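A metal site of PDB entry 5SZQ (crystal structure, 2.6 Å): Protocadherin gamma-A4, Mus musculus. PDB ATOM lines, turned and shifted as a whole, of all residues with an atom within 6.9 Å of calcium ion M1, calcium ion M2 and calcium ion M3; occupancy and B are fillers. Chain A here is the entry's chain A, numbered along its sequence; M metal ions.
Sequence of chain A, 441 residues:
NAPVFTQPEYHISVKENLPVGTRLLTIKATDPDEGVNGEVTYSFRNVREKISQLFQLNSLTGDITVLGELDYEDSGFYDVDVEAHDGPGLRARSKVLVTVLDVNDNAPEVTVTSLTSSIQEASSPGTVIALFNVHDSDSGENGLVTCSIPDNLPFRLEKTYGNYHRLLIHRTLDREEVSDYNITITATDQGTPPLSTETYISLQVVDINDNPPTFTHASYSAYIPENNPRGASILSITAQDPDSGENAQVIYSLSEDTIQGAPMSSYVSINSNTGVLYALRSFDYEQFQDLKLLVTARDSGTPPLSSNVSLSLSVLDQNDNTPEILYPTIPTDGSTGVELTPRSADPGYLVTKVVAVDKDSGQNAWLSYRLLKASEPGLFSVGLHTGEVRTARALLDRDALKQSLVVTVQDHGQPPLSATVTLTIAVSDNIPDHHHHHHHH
Of the 26 residues printed, 6 come within 4 Å of calcium ion M1. The nearest printed residue that does not touch calcium ion M1 is Arg 175 (4.4 Å).
The side-chain carboxylate (OE2) of Glu 176 sits close to the guanidinium group (NH1) of Arg 175. The backbone NH (N) of Glu 121 sits at hydrogen-bond distance from the backbone carbonyl oxygen (O) of Val 206 (3.4 Å). The side-chain carboxylate (OD2) of Asp 174 lies close to the side-chain carboxylate (OE1) of Glu 176 (2.7 Å). The backbone carbonyl oxygen of Glu 121 lies close to the backbone carbonyl oxygen of Leu 173. The guanidinium group of Arg 175 sits close to the side-chain carboxylate of Asp 207, 3.8 Å away. OD1 of Asp 299 sits at hydrogen-bond distance from N of Leu 305 (2.6 Å). N of Ser 244 lies within hydrogen-bond range of OD2 of Asp 207 (3.2 Å). OD1 of Asn 211 sits close to OD1 of Asp 210 (2.9 Å).
Calcium ion M2 is bound by OD2 of Asp 210 (2.5 Å), OD2 of Asp 174 (2.5 Å) and OE1 of Glu 121 (2.6 Å). Calcium ion M2 has three donor atoms within binding distance. Slightly farther from calcium ion M2 lies OE1 of Glu 176 (3.1 Å). Slightly farther from calcium ion M2 lies OD1 of Asp 174 (3.1 Å).
OE2 of Glu 176 binds calcium ion M1, 2.3 Å away. The side-chain carboxylate (OD1) of Asp 207 is bound to calcium ion M1, 2.3 Å away. O of Ile 208 is bound to calcium ion M1, 2.4 Å away. The side-chain carboxylate (OE2) of Glu 121 is bound to calcium ion M1, at 2.6 Å. The side-chain carboxylate (OD1) of Asp 243 binds calcium ion M1, 2.8 Å away. Calcium ion M1 has five donor atoms within binding distance. Slightly farther from calcium ion M1 lies OD1 of Asp 210 (3.0 Å). Slightly farther from calcium ion M1 lies OE1 of Glu 176 (3.0 Å).
The nearest printed residue that does not touch calcium ion M3 is Pro 212 (4.3 Å).
Calcium ion M3 is bound by the side-chain amide oxygen (OD1) of Asn 209 (2.4 Å), the backbone carbonyl oxygen (O) of Asn 211 (2.4 Å), the backbone carbonyl oxygen (O) of Asn 247 (2.4 Å), the side-chain carboxylate (OD2) of Asp 241 (2.5 Å), the side-chain carboxylate (OD2) of Asp 299 (2.6 Å) and the side-chain carboxylate (OD2) of Asp 243 (2.8 Å). Slightly farther from calcium ion M3 lies OD1 of Asp 241 (2.9 Å).
Of the 26 residues printed, 5 come within 4 Å of calcium ion M2.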
ATOM      1  N   GLU A 121      18.892  25.243  20.269  1.00  0.00           N
ATOM      2  CA  GLU A 121      20.161  24.636  20.671  1.00  0.00           C
ATOM      3  C   GLU A 121      20.445  24.901  22.143  1.00  0.00           C
ATOM      4  O   GLU A 121      20.439  23.968  22.956  1.00  0.00           O
ATOM      5  CB  GLU A 121      21.289  25.181  19.782  1.00  0.00           C
ATOM      6  CG  GLU A 121      22.620  24.466  19.973  1.00  0.00           C
ATOM      7  CD  GLU A 121      23.711  24.976  19.057  1.00  0.00           C
ATOM      8  OE1 GLU A 121      24.807  25.291  19.559  1.00  0.00           O
ATOM      9  OE2 GLU A 121      23.463  25.061  17.831  1.00  0.00           O
ATOM     10  N   LEU A 173      20.968  20.051  25.175  1.00  0.00           N
ATOM     11  CA  LEU A 173      21.058  19.665  23.778  1.00  0.00           C
ATOM     12  C   LEU A 173      21.950  20.644  23.023  1.00  0.00           C
ATOM     13  O   LEU A 173      21.998  21.837  23.341  1.00  0.00           O
ATOM     14  CB  LEU A 173      19.656  19.619  23.156  1.00  0.00           C
ATOM     15  CG  LEU A 173      19.441  18.945  21.797  1.00  0.00           C
ATOM     16  CD1 LEU A 173      19.693  19.924  20.673  1.00  0.00           C
ATOM     17  CD2 LEU A 173      20.311  17.700  21.657  1.00  0.00           C
ATOM     18  N   ASP A 174      22.674  20.134  22.014  1.00  0.00           N
ATOM     19  CA  ASP A 174      23.580  20.940  21.201  1.00  0.00           C
ATOM     20  C   ASP A 174      23.525  20.439  19.762  1.00  0.00           C
ATOM     21  O   ASP A 174      23.773  19.255  19.515  1.00  0.00           O
ATOM     22  CB  ASP A 174      25.019  20.879  21.738  1.00  0.00           C
ATOM     23  CG  ASP A 174      25.993  21.729  20.912  1.00  0.00           C
ATOM     24  OD1 ASP A 174      27.222  21.504  21.015  1.00  0.00           O
ATOM     25  OD2 ASP A 174      25.522  22.617  20.172  1.00  0.00           O
ATOM     26  N   ARG A 175      23.222  21.339  18.835  1.00  0.00           N
ATOM     27  CA  ARG A 175      22.970  20.942  17.445  1.00  0.00           C
ATOM     28  C   ARG A 175      24.217  20.375  16.776  1.00  0.00           C
ATOM     29  O   ARG A 175      24.105  19.555  15.858  1.00  0.00           O
ATOM     30  CB  ARG A 175      22.437  22.145  16.667  1.00  0.00           C
ATOM     31  CG  ARG A 175      22.156  21.885  15.216  1.00  0.00           C
ATOM     32  CD  ARG A 175      23.228  22.523  14.362  1.00  0.00           C
ATOM     33  NE  ARG A 175      23.523  21.741  13.167  1.00  0.00           N
ATOM     34  CZ  ARG A 175      24.546  21.980  12.348  1.00  0.00           C
ATOM     35  NH1 ARG A 175      25.369  22.985  12.606  1.00  0.00           N
ATOM     36  NH2 ARG A 175      24.750  21.210  11.290  1.00  0.00           N
ATOM     37  N   GLU A 176      25.412  20.777  17.221  1.00  0.00           N
ATOM     38  CA  GLU A 176      26.646  20.377  16.557  1.00  0.00           C
ATOM     39  C   GLU A 176      26.992  18.897  16.744  1.00  0.00           C
ATOM     40  O   GLU A 176      27.984  18.448  16.176  1.00  0.00           O
ATOM     41  CB  GLU A 176      27.818  21.246  17.034  1.00  0.00           C
ATOM     42  CG  GLU A 176      27.895  22.610  16.366  1.00  0.00           C
ATOM     43  CD  GLU A 176      26.643  23.440  16.576  1.00  0.00           C
ATOM     44  OE1 GLU A 176      26.197  23.558  17.733  1.00  0.00           O
ATOM     45  OE2 GLU A 176      26.098  23.950  15.574  1.00  0.00           O
ATOM     46  N   GLU A 177      26.213  18.145  17.530  1.00  0.00           N
ATOM     47  CA  GLU A 177      26.459  16.719  17.694  1.00  0.00           C
ATOM     48  C   GLU A 177      25.688  15.900  16.658  1.00  0.00           C
ATOM     49  O   GLU A 177      26.285  15.113  15.902  1.00  0.00           O
ATOM     50  CB  GLU A 177      26.098  16.264  19.110  1.00  0.00           C
ATOM     51  CG  GLU A 177      27.213  16.419  20.138  1.00  0.00           C
ATOM     52  CD  GLU A 177      27.524  17.872  20.436  1.00  0.00           C
ATOM     53  OE1 GLU A 177      28.687  18.173  20.786  1.00  0.00           O
ATOM     54  OE2 GLU A 177      26.609  18.716  20.312  1.00  0.00           O
ATOM     55  N   VAL A 206      17.016  23.268  16.185  1.00  0.00           N
ATOM     56  CA  VAL A 206      17.316  24.664  15.859  1.00  0.00           C
ATOM     57  C   VAL A 206      18.801  24.917  16.081  1.00  0.00           C
ATOM     58  O   VAL A 206      19.417  24.371  17.011  1.00  0.00           O
ATOM     59  CB  VAL A 206      16.439  25.605  16.708  1.00  0.00           C
ATOM     60  CG1 VAL A 206      16.691  27.052  16.343  1.00  0.00           C
ATOM     61  CG2 VAL A 206      14.971  25.246  16.536  1.00  0.00           C
ATOM     62  N   ASP A 207      19.393  25.739  15.206  1.00  0.00           N
ATOM     63  CA  ASP A 207      20.830  25.976  15.164  1.00  0.00           C
ATOM     64  C   ASP A 207      21.111  27.435  15.525  1.00  0.00           C
ATOM     65  O   ASP A 207      20.759  28.341  14.763  1.00  0.00           O
ATOM     66  CB  ASP A 207      21.384  25.638  13.783  1.00  0.00           C
ATOM     67  CG  ASP A 207      22.824  26.053  13.603  1.00  0.00           C
ATOM     68  OD1 ASP A 207      23.633  25.790  14.518  1.00  0.00           O
ATOM     69  OD2 ASP A 207      23.165  26.638  12.558  1.00  0.00           O
ATOM     70  N   ILE A 208      21.739  27.654  16.692  1.00  0.00           N
ATOM     71  CA  ILE A 208      22.185  28.984  17.106  1.00  0.00           C
ATOM     72  C   ILE A 208      23.586  29.222  16.554  1.00  0.00           C
ATOM     73  O   ILE A 208      24.384  28.296  16.390  1.00  0.00           O
ATOM     74  CB  ILE A 208      22.168  29.136  18.649  1.00  0.00           C
ATOM     75  CG1 ILE A 208      20.761  28.909  19.194  1.00  0.00           C
ATOM     76  CG2 ILE A 208      22.665  30.518  19.079  1.00  0.00           C
ATOM     77  CD1 ILE A 208      20.633  29.265  20.661  1.00  0.00           C
ATOM     78  N   ASN A 209      23.880  30.492  16.249  1.00  0.00           N
ATOM     79  CA  ASN A 209      25.207  30.895  15.804  1.00  0.00           C
ATOM     80  C   ASN A 209      26.089  31.137  17.025  1.00  0.00           C
ATOM     81  O   ASN A 209      26.363  32.270  17.433  1.00  0.00           O
ATOM     82  CB  ASN A 209      25.111  32.148  14.934  1.00  0.00           C
ATOM     83  CG  ASN A 209      26.422  32.509  14.273  1.00  0.00           C
ATOM     84  OD1 ASN A 209      27.257  31.638  14.023  1.00  0.00           O
ATOM     85  ND2 ASN A 209      26.608  33.796  13.993  1.00  0.00           N
ATOM     86  N   ASP A 210      26.554  30.040  17.621  1.00  0.00           N
ATOM     87  CA  ASP A 210      27.376  30.098  18.827  1.00  0.00           C
ATOM     88  C   ASP A 210      28.814  29.658  18.592  1.00  0.00           C
ATOM     89  O   ASP A 210      29.624  29.746  19.519  1.00  0.00           O
ATOM     90  CB  ASP A 210      26.741  29.251  19.943  1.00  0.00           C
ATOM     91  CG  ASP A 210      26.662  27.780  19.593  1.00  0.00           C
ATOM     92  OD1 ASP A 210      26.705  27.446  18.390  1.00  0.00           O
ATOM     93  OD2 ASP A 210      26.540  26.954  20.525  1.00  0.00           O
ATOM     94  N   ASN A 211      29.154  29.181  17.388  1.00  0.00           N
ATOM     95  CA  ASN A 211      30.513  28.827  17.034  1.00  0.00           C
ATOM     96  C   ASN A 211      31.059  29.783  15.976  1.00  0.00           C
ATOM     97  O   ASN A 211      30.334  30.131  15.031  1.00  0.00           O
ATOM     98  CB  ASN A 211      30.606  27.397  16.511  1.00  0.00           C
ATOM     99  CG  ASN A 211      30.201  26.359  17.543  1.00  0.00           C
ATOM    100  OD1 ASN A 211      29.467  26.660  18.483  1.00  0.00           O
ATOM    101  ND2 ASN A 211      30.664  25.131  17.360  1.00  0.00           N
ATOM    102  N   PRO A 212      32.297  30.242  16.100  1.00  0.00           N
ATOM    103  CA  PRO A 212      32.889  31.077  15.058  1.00  0.00           C
ATOM    104  C   PRO A 212      33.590  30.226  14.013  1.00  0.00           C
ATOM    105  O   PRO A 212      33.813  29.028  14.228  1.00  0.00           O
ATOM    106  CB  PRO A 212      33.898  31.936  15.837  1.00  0.00           C
ATOM    107  CG  PRO A 212      34.332  31.033  16.947  1.00  0.00           C
ATOM    108  CD  PRO A 212      33.135  30.195  17.312  1.00  0.00           C
ATOM    109  N   PRO A 213      33.928  30.807  12.862  1.00  0.00           N
ATOM    110  CA  PRO A 213      34.765  30.083  11.885  1.00  0.00           C
ATOM    111  C   PRO A 213      36.203  29.985  12.363  1.00  0.00           C
ATOM    112  O   PRO A 213      36.786  30.976  12.819  1.00  0.00           O
ATOM    113  CB  PRO A 213      34.637  30.923  10.607  1.00  0.00           C
ATOM    114  CG  PRO A 213      34.233  32.280  11.083  1.00  0.00           C
ATOM    115  CD  PRO A 213      33.396  32.068  12.307  1.00  0.00           C
ATOM    116  N   ASP A 241      33.352  26.500   9.830  1.00  0.00           N
ATOM    117  CA  ASP A 241      32.405  26.832  10.872  1.00  0.00           C
ATOM    118  C   ASP A 241      31.505  25.637  11.154  1.00  0.00           C
ATOM    119  O   ASP A 241      30.767  25.197  10.254  1.00  0.00           O
ATOM    120  CB  ASP A 241      31.559  28.047  10.479  1.00  0.00           C
ATOM    121  CG  ASP A 241      30.688  28.544  11.625  1.00  0.00           C
ATOM    122  OD1 ASP A 241      31.217  28.648  12.758  1.00  0.00           O
ATOM    123  OD2 ASP A 241      29.495  28.809  11.412  1.00  0.00           O
ATOM    124  N   PRO A 242      31.523  25.073  12.369  1.00  0.00           N
ATOM    125  CA  PRO A 242      30.749  23.851  12.639  1.00  0.00           C
ATOM    126  C   PRO A 242      29.238  24.056  12.639  1.00  0.00           C
ATOM    127  O   PRO A 242      28.506  23.092  12.913  1.00  0.00           O
ATOM    128  CB  PRO A 242      31.241  23.423  14.033  1.00  0.00           C
ATOM    129  CG  PRO A 242      32.538  24.153  14.244  1.00  0.00           C
ATOM    130  CD  PRO A 242      32.386  25.440  13.504  1.00  0.00           C
ATOM    131  N   ASP A 243      28.734  25.261  12.352  1.00  0.00           N
ATOM    132  CA  ASP A 243      27.303  25.503  12.378  1.00  0.00           C
ATOM    133  C   ASP A 243      26.654  25.083  11.061  1.00  0.00           C
ATOM    134  O   ASP A 243      27.082  24.119  10.429  1.00  0.00           O
ATOM    135  CB  ASP A 243      27.002  26.970  12.673  1.00  0.00           C
ATOM    136  CG  ASP A 243      27.495  27.407  14.040  1.00  0.00           C
ATOM    137  OD1 ASP A 243      27.630  26.526  14.926  1.00  0.00           O
ATOM    138  OD2 ASP A 243      27.737  28.611  14.238  1.00  0.00           O
ATOM    139  N   SER A 244      25.614  25.801  10.643  1.00  0.00           N
ATOM    140  CA  SER A 244      24.886  25.437   9.436  1.00  0.00           C
ATOM    141  C   SER A 244      24.162  26.670   8.903  1.00  0.00           C
ATOM    142  O   SER A 244      23.946  27.648   9.622  1.00  0.00           O
ATOM    143  CB  SER A 244      23.898  24.297   9.702  1.00  0.00           C
ATOM    144  OG  SER A 244      23.306  23.827   8.508  1.00  0.00           O
ATOM    145  N   GLU A 246      23.034  30.061   7.138  1.00  0.00           N
ATOM    146  CA  GLU A 246      23.654  31.375   7.082  1.00  0.00           C
ATOM    147  C   GLU A 246      24.723  31.529   8.145  1.00  0.00           C
ATOM    148  O   GLU A 246      25.789  32.106   7.898  1.00  0.00           O
ATOM    149  CB  GLU A 246      22.587  32.469   7.221  1.00  0.00           C
ATOM    150  CG  GLU A 246      22.312  33.267   5.948  1.00  0.00           C
ATOM    151  CD  GLU A 246      21.452  34.480   6.217  1.00  0.00           C
ATOM    152  OE1 GLU A 246      21.215  34.798   7.402  1.00  0.00           O
ATOM    153  OE2 GLU A 246      20.989  35.122   5.248  1.00  0.00           O
ATOM    154  N   ASN A 247      24.478  30.995   9.340  1.00  0.00           N
ATOM    155  CA  ASN A 247      25.408  31.093  10.467  1.00  0.00           C
ATOM    156  C   ASN A 247      26.727  30.373  10.237  1.00  0.00           C
ATOM    157  O   ASN A 247      27.586  30.411  11.119  1.00  0.00           O
ATOM    158  CB  ASN A 247      24.734  30.561  11.730  1.00  0.00           C
ATOM    159  CG  ASN A 247      23.467  31.307  12.077  1.00  0.00           C
ATOM    160  OD1 ASN A 247      23.377  32.522  11.899  1.00  0.00           O
ATOM    161  ND2 ASN A 247      22.472  30.589  12.595  1.00  0.00           N
ATOM    162  N   ALA A 248      26.913  29.719   9.089  1.00  0.00           N
ATOM    163  CA  ALA A 248      28.127  28.943   8.837  1.00  0.00           C
ATOM    164  C   ALA A 248      28.866  29.313   7.566  1.00  0.00           C
ATOM    165  O   ALA A 248      29.948  28.767   7.324  1.00  0.00           O
ATOM    166  CB  ALA A 248      27.815  27.444   8.786  1.00  0.00           C
ATOM    167  N   GLN A 249      28.329  30.207   6.741  1.00  0.00           N
ATOM    168  CA  GLN A 249      29.074  30.714   5.601  1.00  0.00           C
ATOM    169  C   GLN A 249      30.326  31.437   6.068  1.00  0.00           C
ATOM    170  O   GLN A 249      30.370  31.985   7.168  1.00  0.00           O
ATOM    171  CB  GLN A 249      28.203  31.666   4.772  1.00  0.00           C
ATOM    172  CG  GLN A 249      26.925  31.031   4.234  1.00  0.00           C
ATOM    173  CD  GLN A 249      26.092  32.026   3.444  1.00  0.00           C
ATOM    174  OE1 GLN A 249      26.488  33.175   3.255  1.00  0.00           O
ATOM    175  NE2 GLN A 249      24.938  31.580   2.968  1.00  0.00           N
ATOM    176  N   ARG A 298      34.418  35.966   8.666  1.00  0.00           N
ATOM    177  CA  ARG A 298      33.154  36.132   9.370  1.00  0.00           C
ATOM    178  C   ARG A 298      32.091  35.207   8.774  1.00  0.00           C
ATOM    179  O   ARG A 298      32.335  34.503   7.791  1.00  0.00           O
ATOM    180  CB  ARG A 298      32.692  37.598   9.310  1.00  0.00           C
ATOM    181  CG  ARG A 298      32.302  38.076   7.916  1.00  0.00           C
ATOM    182  CD  ARG A 298      31.685  39.470   7.964  1.00  0.00           C
ATOM    183  NE  ARG A 298      31.340  39.954   6.631  1.00  0.00           N
ATOM    184  CZ  ARG A 298      30.177  39.733   6.030  1.00  0.00           C
ATOM    185  NH1 ARG A 298      29.949  40.209   4.809  1.00  0.00           N
ATOM    186  NH2 ARG A 298      29.230  39.035   6.644  1.00  0.00           N
ATOM    187  N   ASP A 299      30.907  35.205   9.390  1.00  0.00           N
ATOM    188  CA  ASP A 299      29.760  34.467   8.888  1.00  0.00           C
ATOM    189  C   ASP A 299      28.620  35.428   8.578  1.00  0.00           C
ATOM    190  O   ASP A 299      28.617  36.588   9.001  1.00  0.00           O
ATOM    191  CB  ASP A 299      29.296  33.382   9.875  1.00  0.00           C
ATOM    192  CG  ASP A 299      28.879  33.935  11.234  1.00  0.00           C
ATOM    193  OD1 ASP A 299      28.887  35.160  11.432  1.00  0.00           O
ATOM    194  OD2 ASP A 299      28.537  33.116  12.117  1.00  0.00           O
ATOM    195  N   SER A 300      27.652  34.931   7.812  1.00  0.00           N
ATOM    196  CA  SER A 300      26.480  35.726   7.449  1.00  0.00           C
ATOM    197  C   SER A 300      25.492  35.724   8.611  1.00  0.00           C
ATOM    198  O   SER A 300      25.775  35.254   9.710  1.00  0.00           O
ATOM    199  CB  SER A 300      25.874  35.194   6.152  1.00  0.00           C
ATOM    200  OG  SER A 300      26.823  35.198   5.098  1.00  0.00           O
ATOM    201  N   LEU A 305      29.903  36.719  13.192  1.00  0.00           N
ATOM    202  CA  LEU A 305      30.878  36.166  14.118  1.00  0.00           C
ATOM    203  C   LEU A 305      32.120  35.782  13.326  1.00  0.00           C
ATOM    204  O   LEU A 305      32.036  34.987  12.383  1.00  0.00           O
ATOM    205  CB  LEU A 305      30.312  34.941  14.845  1.00  0.00           C
ATOM    206  CG  LEU A 305      31.176  34.227  15.891  1.00  0.00           C
ATOM    207  CD1 LEU A 305      31.810  35.210  16.862  1.00  0.00           C
ATOM    208  CD2 LEU A 305      30.362  33.182  16.653  1.00  0.00           C
HETATM  209 CA    CA M   1      25.223  26.002  16.209  1.00  0.00          CA
HETATM  210 CA    CA M   2      27.129  24.566  20.477  1.00  0.00          CA
HETATM  211 CA    CA M   3      29.149  30.698  12.981  1.00  0.00          CA
